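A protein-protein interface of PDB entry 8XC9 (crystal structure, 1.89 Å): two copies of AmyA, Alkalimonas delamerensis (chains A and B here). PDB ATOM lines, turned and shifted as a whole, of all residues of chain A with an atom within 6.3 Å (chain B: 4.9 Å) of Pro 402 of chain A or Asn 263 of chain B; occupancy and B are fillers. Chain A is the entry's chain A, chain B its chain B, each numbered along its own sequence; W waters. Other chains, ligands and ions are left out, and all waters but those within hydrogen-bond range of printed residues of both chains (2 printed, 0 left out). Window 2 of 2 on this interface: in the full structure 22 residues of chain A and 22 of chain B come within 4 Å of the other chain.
OE1 of Glu 368 of chain A lies within hydrogen-bond range of ND2 of Asn 263 of chain B, 2.8 Å away. The indole nitrogen (NE1) of Trp 267 of chain B is in hydrogen-bond range of the side-chain carboxylate (OE1) of Glu 368 of chain A (2.5 Å).
OE2 of Glu 368 of chain A is in hydrogen-bond range of N of Gly 403 of chain A, 3.1 Å away. N of Glu 368 of chain A lies within hydrogen-bond range of OH of Tyr 416 of chain A (3.1 Å). The guanidinium group (NE) of Arg 418 of chain A is in hydrogen-bond range of the backbone carbonyl oxygen (O) of Gly 401 of chain A (3.0 Å). The backbone carbonyl oxygen (O) of Pro 402 of chain A is in hydrogen-bond range of the backbone NH (N) of Glu 419 of chain A (2.8 Å). OE2 of Glu 419 of chain A is in hydrogen-bond range of NE2 of His 404 of chain A, at 2.8 Å.
Among the printed residues, pairs that only touch across the chains: Gly 401 of chain A with Trp 267 of chain B, Leu 421 of chain A with Trp 267 of chain B, Arg 418 of chain A with Trp 267 of chain B, Pro 402 of chain A with Trp 267 of chain B, Glu 419 of chain A with His 264 of chain B and Pro 402 of chain A with Asn 263 of chain B.
Pro 402 of chain A touches just these residues of chain B: Asn 263 (3.96 Å) and Trp 267 (3.6 Å). Of the printed residues of chain A, His 264 of chain B touches Glu 419. Of the printed residues of chain B, Gly 401 of chain A touches Trp 267. Of the printed residues of chain B, Leu 421 of chain A touches Trp 267 (3.6 Å). Of the printed residues of chain B, Arg 418 of chain A touches Trp 267. Gln 266 of chain B touches none of the printed residues of chain A. The nearest residue of chain B that does not touch Pro 402 of chain A is His 264 of chain B (4.2 Å). The nearest printed residue of chain B that does not touch Leu 421 of chain A is Gln 266 of chain B (7.1 Å).
No position is printed for both chains. Of the 8 pairs that touch across the chains among the printed residues, none has its exchanged pair printed and touching as well.
Water W1 lies within hydrogen-bond range of the backbone carbonyl oxygen (O) of Gly 403 of chain A (2.8 Å) and the side-chain amide nitrogen (ND2) of Asn 263 of chain B (3.2 Å). Water W2 bridges OE2 of Glu 419 of chain A and ND1 of His 264 of chain B.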
ATOM      1  N   GLU A 368       3.751  -1.760   1.469  1.00  0.00           N
ATOM      2  CA  GLU A 368       4.730  -1.317   0.482  1.00  0.00           C
ATOM      3  C   GLU A 368       4.300  -0.067  -0.290  1.00  0.00           C
ATOM      4  O   GLU A 368       5.163   0.666  -0.778  1.00  0.00           O
ATOM      5  CB  GLU A 368       5.022  -2.460  -0.499  1.00  0.00           C
ATOM      6  CG  GLU A 368       5.636  -2.048  -1.831  1.00  0.00           C
ATOM      7  CD  GLU A 368       5.998  -3.234  -2.718  1.00  0.00           C
ATOM      8  OE1 GLU A 368       7.070  -3.199  -3.362  1.00  0.00           O
ATOM      9  OE2 GLU A 368       5.212  -4.201  -2.757  1.00  0.00           O
ATOM     10  N   HIS A 369       3.006   0.194  -0.430  1.00  0.00           N
ATOM     11  CA  HIS A 369       2.552   1.314  -1.244  1.00  0.00           C
ATOM     12  C   HIS A 369       2.134   2.486  -0.367  1.00  0.00           C
ATOM     13  O   HIS A 369       1.784   2.327   0.803  1.00  0.00           O
ATOM     14  CB  HIS A 369       1.388   0.893  -2.138  1.00  0.00           C
ATOM     15  CG  HIS A 369       1.566  -0.467  -2.729  1.00  0.00           C
ATOM     16  ND1 HIS A 369       2.404  -0.707  -3.797  1.00  0.00           N
ATOM     17  CD2 HIS A 369       1.050  -1.667  -2.374  1.00  0.00           C
ATOM     18  CE1 HIS A 369       2.376  -1.995  -4.089  1.00  0.00           C
ATOM     19  NE2 HIS A 369       1.570  -2.601  -3.233  1.00  0.00           N
ATOM     20  N   TYR A 400      11.236  -2.799   3.805  1.00  0.00           N
ATOM     21  CA  TYR A 400      11.857  -2.695   2.488  1.00  0.00           C
ATOM     22  C   TYR A 400      11.702  -3.998   1.723  1.00  0.00           C
ATOM     23  O   TYR A 400      11.453  -5.059   2.301  1.00  0.00           O
ATOM     24  CB  TYR A 400      13.340  -2.319   2.608  1.00  0.00           C
ATOM     25  CG  TYR A 400      13.494  -0.947   3.208  1.00  0.00           C
ATOM     26  CD1 TYR A 400      13.460   0.189   2.398  1.00  0.00           C
ATOM     27  CD2 TYR A 400      13.612  -0.785   4.577  1.00  0.00           C
ATOM     28  CE1 TYR A 400      13.579   1.457   2.943  1.00  0.00           C
ATOM     29  CE2 TYR A 400      13.724   0.470   5.137  1.00  0.00           C
ATOM     30  CZ  TYR A 400      13.704   1.591   4.309  1.00  0.00           C
ATOM     31  OH  TYR A 400      13.812   2.844   4.864  1.00  0.00           O
ATOM     32  N   GLY A 401      11.876  -3.906   0.402  1.00  0.00           N
ATOM     33  CA  GLY A 401      11.736  -5.051  -0.465  1.00  0.00           C
ATOM     34  C   GLY A 401      10.278  -5.334  -0.748  1.00  0.00           C
ATOM     35  O   GLY A 401       9.384  -4.649  -0.254  1.00  0.00           O
ATOM     36  N   PRO A 402      10.014  -6.344  -1.570  1.00  0.00           N
ATOM     37  CA  PRO A 402       8.637  -6.596  -2.007  1.00  0.00           C
ATOM     38  C   PRO A 402       7.696  -6.943  -0.864  1.00  0.00           C
ATOM     39  O   PRO A 402       8.063  -7.634   0.094  1.00  0.00           O
ATOM     40  CB  PRO A 402       8.793  -7.771  -2.980  1.00  0.00           C
ATOM     41  CG  PRO A 402      10.190  -7.642  -3.491  1.00  0.00           C
ATOM     42  CD  PRO A 402      11.002  -7.094  -2.360  1.00  0.00           C
ATOM     43  N   GLY A 403       6.459  -6.486  -0.995  1.00  0.00           N
ATOM     44  CA  GLY A 403       5.399  -6.830  -0.069  1.00  0.00           C
ATOM     45  C   GLY A 403       4.554  -7.984  -0.573  1.00  0.00           C
ATOM     46  O   GLY A 403       4.421  -8.195  -1.775  1.00  0.00           O
ATOM     47  N   HIS A 404       3.985  -8.739   0.365  1.00  0.00           N
ATOM     48  CA  HIS A 404       3.093  -9.837   0.042  1.00  0.00           C
ATOM     49  C   HIS A 404       1.908  -9.844   0.992  1.00  0.00           C
ATOM     50  O   HIS A 404       2.091  -9.796   2.214  1.00  0.00           O
ATOM     51  CB  HIS A 404       3.833 -11.197   0.109  1.00  0.00           C
ATOM     52  CG  HIS A 404       5.138 -11.215  -0.627  1.00  0.00           C
ATOM     53  ND1 HIS A 404       5.236 -11.590  -1.953  1.00  0.00           N
ATOM     54  CD2 HIS A 404       6.395 -10.893  -0.236  1.00  0.00           C
ATOM     55  CE1 HIS A 404       6.496 -11.495  -2.342  1.00  0.00           C
ATOM     56  NE2 HIS A 404       7.219 -11.064  -1.325  1.00  0.00           N
ATOM     57  N   TYR A 416       0.778  -9.531   6.900  1.00  0.00           N
ATOM     58  CA  TYR A 416       1.416  -8.916   5.751  1.00  0.00           C
ATOM     59  C   TYR A 416       2.914  -9.074   5.927  1.00  0.00           C
ATOM     60  O   TYR A 416       3.409  -9.062   7.052  1.00  0.00           O
ATOM     61  CB  TYR A 416       1.050  -7.418   5.649  1.00  0.00           C
ATOM     62  CG  TYR A 416       1.608  -6.722   4.422  1.00  0.00           C
ATOM     63  CD1 TYR A 416       2.915  -6.246   4.401  1.00  0.00           C
ATOM     64  CD2 TYR A 416       0.831  -6.539   3.284  1.00  0.00           C
ATOM     65  CE1 TYR A 416       3.423  -5.603   3.290  1.00  0.00           C
ATOM     66  CE2 TYR A 416       1.330  -5.886   2.168  1.00  0.00           C
ATOM     67  CZ  TYR A 416       2.631  -5.435   2.175  1.00  0.00           C
ATOM     68  OH  TYR A 416       3.142  -4.787   1.081  1.00  0.00           O
ATOM     69  N   VAL A 417       3.631  -9.175   4.816  1.00  0.00           N
ATOM     70  CA  VAL A 417       5.047  -9.514   4.834  1.00  0.00           C
ATOM     71  C   VAL A 417       5.826  -8.514   4.001  1.00  0.00           C
ATOM     72  O   VAL A 417       5.392  -8.118   2.911  1.00  0.00           O
ATOM     73  CB  VAL A 417       5.293 -10.953   4.311  1.00  0.00           C
ATOM     74  CG1 VAL A 417       6.784 -11.218   4.136  1.00  0.00           C
ATOM     75  CG2 VAL A 417       4.694 -11.963   5.257  1.00  0.00           C
ATOM     76  N   ARG A 418       6.977  -8.104   4.514  1.00  0.00           N
ATOM     77  CA  ARG A 418       7.958  -7.362   3.731  1.00  0.00           C
ATOM     78  C   ARG A 418       9.173  -8.261   3.592  1.00  0.00           C
ATOM     79  O   ARG A 418       9.720  -8.753   4.592  1.00  0.00           O
ATOM     80  CB  ARG A 418       8.335  -6.022   4.368  1.00  0.00           C
ATOM     81  CG  ARG A 418       7.242  -4.938   4.312  1.00  0.00           C
ATOM     82  CD  ARG A 418       6.766  -4.628   2.885  1.00  0.00           C
ATOM     83  NE  ARG A 418       7.733  -3.880   2.085  1.00  0.00           N
ATOM     84  CZ  ARG A 418       7.876  -2.553   2.122  1.00  0.00           C
ATOM     85  NH1 ARG A 418       7.141  -1.826   2.947  1.00  0.00           N
ATOM     86  NH2 ARG A 418       8.768  -1.952   1.342  1.00  0.00           N
ATOM     87  N   GLU A 419       9.552  -8.516   2.348  1.00  0.00           N
ATOM     88  CA  GLU A 419      10.559  -9.513   2.049  1.00  0.00           C
ATOM     89  C   GLU A 419      11.954  -9.053   2.460  1.00  0.00           C
ATOM     90  O   GLU A 419      12.807  -9.896   2.763  1.00  0.00           O
ATOM     91  CB  GLU A 419      10.453  -9.823   0.550  1.00  0.00           C
ATOM     92  CG  GLU A 419      11.394 -10.794  -0.043  1.00  0.00           C
ATOM     93  CD  GLU A 419      11.156 -10.884  -1.544  1.00  0.00           C
ATOM     94  OE1 GLU A 419      12.154 -10.761  -2.289  1.00  0.00           O
ATOM     95  OE2 GLU A 419       9.973 -11.039  -1.960  1.00  0.00           O
ATOM     96  N   GLY A 420      12.191  -7.735   2.540  1.00  0.00           N
ATOM     97  CA  GLY A 420      13.513  -7.238   2.863  1.00  0.00           C
ATOM     98  C   GLY A 420      14.368  -7.055   1.628  1.00  0.00           C
ATOM     99  O   GLY A 420      13.961  -7.330   0.493  1.00  0.00           O
ATOM    100  N   LEU A 421      15.592  -6.579   1.852  1.00  0.00           N
ATOM    101  CA  LEU A 421      16.531  -6.294   0.772  1.00  0.00           C
ATOM    102  C   LEU A 421      17.653  -7.318   0.781  1.00  0.00           C
ATOM    103  O   LEU A 421      18.213  -7.623   1.845  1.00  0.00           O
ATOM    104  CB  LEU A 421      17.122  -4.893   0.897  1.00  0.00           C
ATOM    105  CG  LEU A 421      16.133  -3.753   0.716  1.00  0.00           C
ATOM    106  CD1 LEU A 421      16.772  -2.431   1.119  1.00  0.00           C
ATOM    107  CD2 LEU A 421      15.625  -3.719  -0.711  1.00  0.00           C
ATOM    108  N   THR B 258       3.205 -10.783 -13.747  1.00  0.00           N
ATOM    109  CA  THR B 258       3.901  -9.655 -14.350  1.00  0.00           C
ATOM    110  C   THR B 258       4.256  -8.627 -13.284  1.00  0.00           C
ATOM    111  O   THR B 258       5.418  -8.216 -13.151  1.00  0.00           O
ATOM    112  CB  THR B 258       3.035  -9.011 -15.448  1.00  0.00           C
ATOM    113  OG1 THR B 258       2.626  -9.991 -16.411  1.00  0.00           O
ATOM    114  CG2 THR B 258       3.800  -7.889 -16.170  1.00  0.00           C
ATOM    115  N   ARG B 259       3.261  -8.229 -12.494  1.00  0.00           N
ATOM    116  CA  ARG B 259       3.487  -7.234 -11.442  1.00  0.00           C
ATOM    117  C   ARG B 259       4.552  -7.696 -10.459  1.00  0.00           C
ATOM    118  O   ARG B 259       5.493  -6.951 -10.146  1.00  0.00           O
ATOM    119  CB  ARG B 259       2.188  -6.945 -10.700  1.00  0.00           C
ATOM    120  CG  ARG B 259       2.417  -6.145  -9.415  1.00  0.00           C
ATOM    121  CD  ARG B 259       1.120  -5.761  -8.761  1.00  0.00           C
ATOM    122  NE  ARG B 259       0.334  -6.924  -8.394  1.00  0.00           N
ATOM    123  CZ  ARG B 259      -0.781  -7.312  -9.008  1.00  0.00           C
ATOM    124  NH1 ARG B 259      -1.267  -6.642 -10.051  1.00  0.00           N
ATOM    125  NH2 ARG B 259      -1.406  -8.392  -8.571  1.00  0.00           N
ATOM    126  N   ASP B 260       4.433  -8.943  -9.987  1.00  0.00           N
ATOM    127  CA  ASP B 260       5.345  -9.469  -8.967  1.00  0.00           C
ATOM    128  C   ASP B 260       6.769  -9.609  -9.493  1.00  0.00           C
ATOM    129  O   ASP B 260       7.729  -9.440  -8.732  1.00  0.00           O
ATOM    130  CB  ASP B 260       4.826 -10.810  -8.457  1.00  0.00           C
ATOM    131  CG  ASP B 260       3.548 -10.672  -7.655  1.00  0.00           C
ATOM    132  OD1 ASP B 260       3.174  -9.524  -7.315  1.00  0.00           O
ATOM    133  OD2 ASP B 260       2.922 -11.709  -7.352  1.00  0.00           O
ATOM    134  N   TRP B 261       6.929  -9.885 -10.792  1.00  0.00           N
ATOM    135  CA  TRP B 261       8.267 -10.039 -11.350  1.00  0.00           C
ATOM    136  C   TRP B 261       8.931  -8.686 -11.564  1.00  0.00           C
ATOM    137  O   TRP B 261      10.116  -8.507 -11.263  1.00  0.00           O
ATOM    138  CB  TRP B 261       8.209 -10.825 -12.663  1.00  0.00           C
ATOM    139  CG  TRP B 261       9.558 -10.945 -13.320  1.00  0.00           C
ATOM    140  CD1 TRP B 261      10.514 -11.890 -13.072  1.00  0.00           C
ATOM    141  CD2 TRP B 261      10.097 -10.085 -14.334  1.00  0.00           C
ATOM    142  NE1 TRP B 261      11.619 -11.667 -13.864  1.00  0.00           N
ATOM    143  CE2 TRP B 261      11.385 -10.564 -14.647  1.00  0.00           C
ATOM    144  CE3 TRP B 261       9.617  -8.949 -15.003  1.00  0.00           C
ATOM    145  CZ2 TRP B 261      12.189  -9.958 -15.611  1.00  0.00           C
ATOM    146  CZ3 TRP B 261      10.420  -8.343 -15.943  1.00  0.00           C
ATOM    147  CH2 TRP B 261      11.690  -8.840 -16.240  1.00  0.00           C
ATOM    148  N   ILE B 262       8.194  -7.740 -12.142  1.00  0.00           N
ATOM    149  CA  ILE B 262       8.690  -6.371 -12.239  1.00  0.00           C
ATOM    150  C   ILE B 262       9.063  -5.852 -10.859  1.00  0.00           C
ATOM    151  O   ILE B 262      10.155  -5.310 -10.644  1.00  0.00           O
ATOM    152  CB  ILE B 262       7.634  -5.467 -12.891  1.00  0.00           C
ATOM    153  CG1 ILE B 262       7.424  -5.853 -14.355  1.00  0.00           C
ATOM    154  CG2 ILE B 262       8.025  -4.002 -12.704  1.00  0.00           C
ATOM    155  CD1 ILE B 262       6.406  -4.966 -15.069  1.00  0.00           C
ATOM    156  N   ASN B 263       8.146  -5.997  -9.908  1.00  0.00           N
ATOM    157  CA  ASN B 263       8.391  -5.457  -8.570  1.00  0.00           C
ATOM    158  C   ASN B 263       9.616  -6.100  -7.938  1.00  0.00           C
ATOM    159  O   ASN B 263      10.399  -5.426  -7.258  1.00  0.00           O
ATOM    160  CB  ASN B 263       7.160  -5.657  -7.685  1.00  0.00           C
ATOM    161  CG  ASN B 263       7.143  -4.714  -6.482  1.00  0.00           C
ATOM    162  OD1 ASN B 263       7.432  -3.523  -6.601  1.00  0.00           O
ATOM    163  ND2 ASN B 263       6.826  -5.256  -5.319  1.00  0.00           N
ATOM    164  N   HIS B 264       9.809  -7.403  -8.175  1.00  0.00           N
ATOM    165  CA  HIS B 264      10.945  -8.103  -7.586  1.00  0.00           C
ATOM    166  C   HIS B 264      12.255  -7.641  -8.197  1.00  0.00           C
ATOM    167  O   HIS B 264      13.229  -7.384  -7.484  1.00  0.00           O
ATOM    168  CB  HIS B 264      10.803  -9.614  -7.771  1.00  0.00           C
ATOM    169  CG  HIS B 264      11.989 -10.369  -7.269  1.00  0.00           C
ATOM    170  ND1 HIS B 264      12.080 -10.826  -5.970  1.00  0.00           N
ATOM    171  CD2 HIS B 264      13.170 -10.664  -7.859  1.00  0.00           C
ATOM    172  CE1 HIS B 264      13.252 -11.409  -5.798  1.00  0.00           C
ATOM    173  NE2 HIS B 264      13.933 -11.322  -6.926  1.00  0.00           N
ATOM    174  N   VAL B 265      12.296  -7.537  -9.526  1.00  0.00           N
ATOM    175  CA  VAL B 265      13.526  -7.147 -10.209  1.00  0.00           C
ATOM    176  C   VAL B 265      13.902  -5.709  -9.866  1.00  0.00           C
ATOM    177  O   VAL B 265      15.088  -5.373  -9.746  1.00  0.00           O
ATOM    178  CB  VAL B 265      13.355  -7.345 -11.723  1.00  0.00           C
ATOM    179  CG1 VAL B 265      14.557  -6.793 -12.469  1.00  0.00           C
ATOM    180  CG2 VAL B 265      13.152  -8.845 -12.031  1.00  0.00           C
ATOM    181  N   GLN B 266      12.906  -4.836  -9.713  1.00  0.00           N
ATOM    182  CA  GLN B 266      13.190  -3.450  -9.356  1.00  0.00           C
ATOM    183  C   GLN B 266      13.784  -3.374  -7.955  1.00  0.00           C
ATOM    184  O   GLN B 266      14.881  -2.838  -7.753  1.00  0.00           O
ATOM    185  CB  GLN B 266      11.916  -2.612  -9.460  1.00  0.00           C
ATOM    186  CG  GLN B 266      12.152  -1.096  -9.385  1.00  0.00           C
ATOM    187  CD  GLN B 266      12.951  -0.573 -10.560  1.00  0.00           C
ATOM    188  OE1 GLN B 266      14.177  -0.730 -10.613  1.00  0.00           O
ATOM    189  NE2 GLN B 266      12.257   0.055 -11.522  1.00  0.00           N
ATOM    190  N   TRP B 267      13.082  -3.938  -6.978  1.00  0.00           N
ATOM    191  CA  TRP B 267      13.605  -3.965  -5.616  1.00  0.00           C
ATOM    192  C   TRP B 267      15.005  -4.575  -5.562  1.00  0.00           C
ATOM    193  O   TRP B 267      15.841  -4.140  -4.764  1.00  0.00           O
ATOM    194  CB  TRP B 267      12.639  -4.732  -4.724  1.00  0.00           C
ATOM    195  CG  TRP B 267      11.561  -3.895  -4.096  1.00  0.00           C
ATOM    196  CD1 TRP B 267      10.210  -3.985  -4.312  1.00  0.00           C
ATOM    197  CD2 TRP B 267      11.742  -2.858  -3.125  1.00  0.00           C
ATOM    198  NE1 TRP B 267       9.542  -3.055  -3.539  1.00  0.00           N
ATOM    199  CE2 TRP B 267      10.461  -2.358  -2.800  1.00  0.00           C
ATOM    200  CE3 TRP B 267      12.860  -2.297  -2.513  1.00  0.00           C
ATOM    201  CZ2 TRP B 267      10.272  -1.332  -1.880  1.00  0.00           C
ATOM    202  CZ3 TRP B 267      12.671  -1.268  -1.597  1.00  0.00           C
ATOM    203  CH2 TRP B 267      11.388  -0.798  -1.293  1.00  0.00           C
ATOM    204  N   HIS B 295       6.330   1.151 -12.288  1.00  0.00           N
ATOM    205  CA  HIS B 295       7.520   0.963 -13.107  1.00  0.00           C
ATOM    206  C   HIS B 295       7.216   0.545 -14.534  1.00  0.00           C
ATOM    207  O   HIS B 295       8.146   0.481 -15.342  1.00  0.00           O
ATOM    208  CB  HIS B 295       8.440  -0.104 -12.508  1.00  0.00           C
ATOM    209  CG  HIS B 295       8.620   0.023 -11.033  1.00  0.00           C
ATOM    210  ND1 HIS B 295       9.134   1.160 -10.444  1.00  0.00           N
ATOM    211  CD2 HIS B 295       8.341  -0.834 -10.024  1.00  0.00           C
ATOM    212  CE1 HIS B 295       9.164   0.996  -9.135  1.00  0.00           C
ATOM    213  NE2 HIS B 295       8.689  -0.205  -8.853  1.00  0.00           N
HETATM  214  O   HOH W   1       5.624  -8.018  -4.306  1.00  0.00           O
HETATM  215  O   HOH W   2       9.571 -11.397  -4.744  1.00  0.00           O
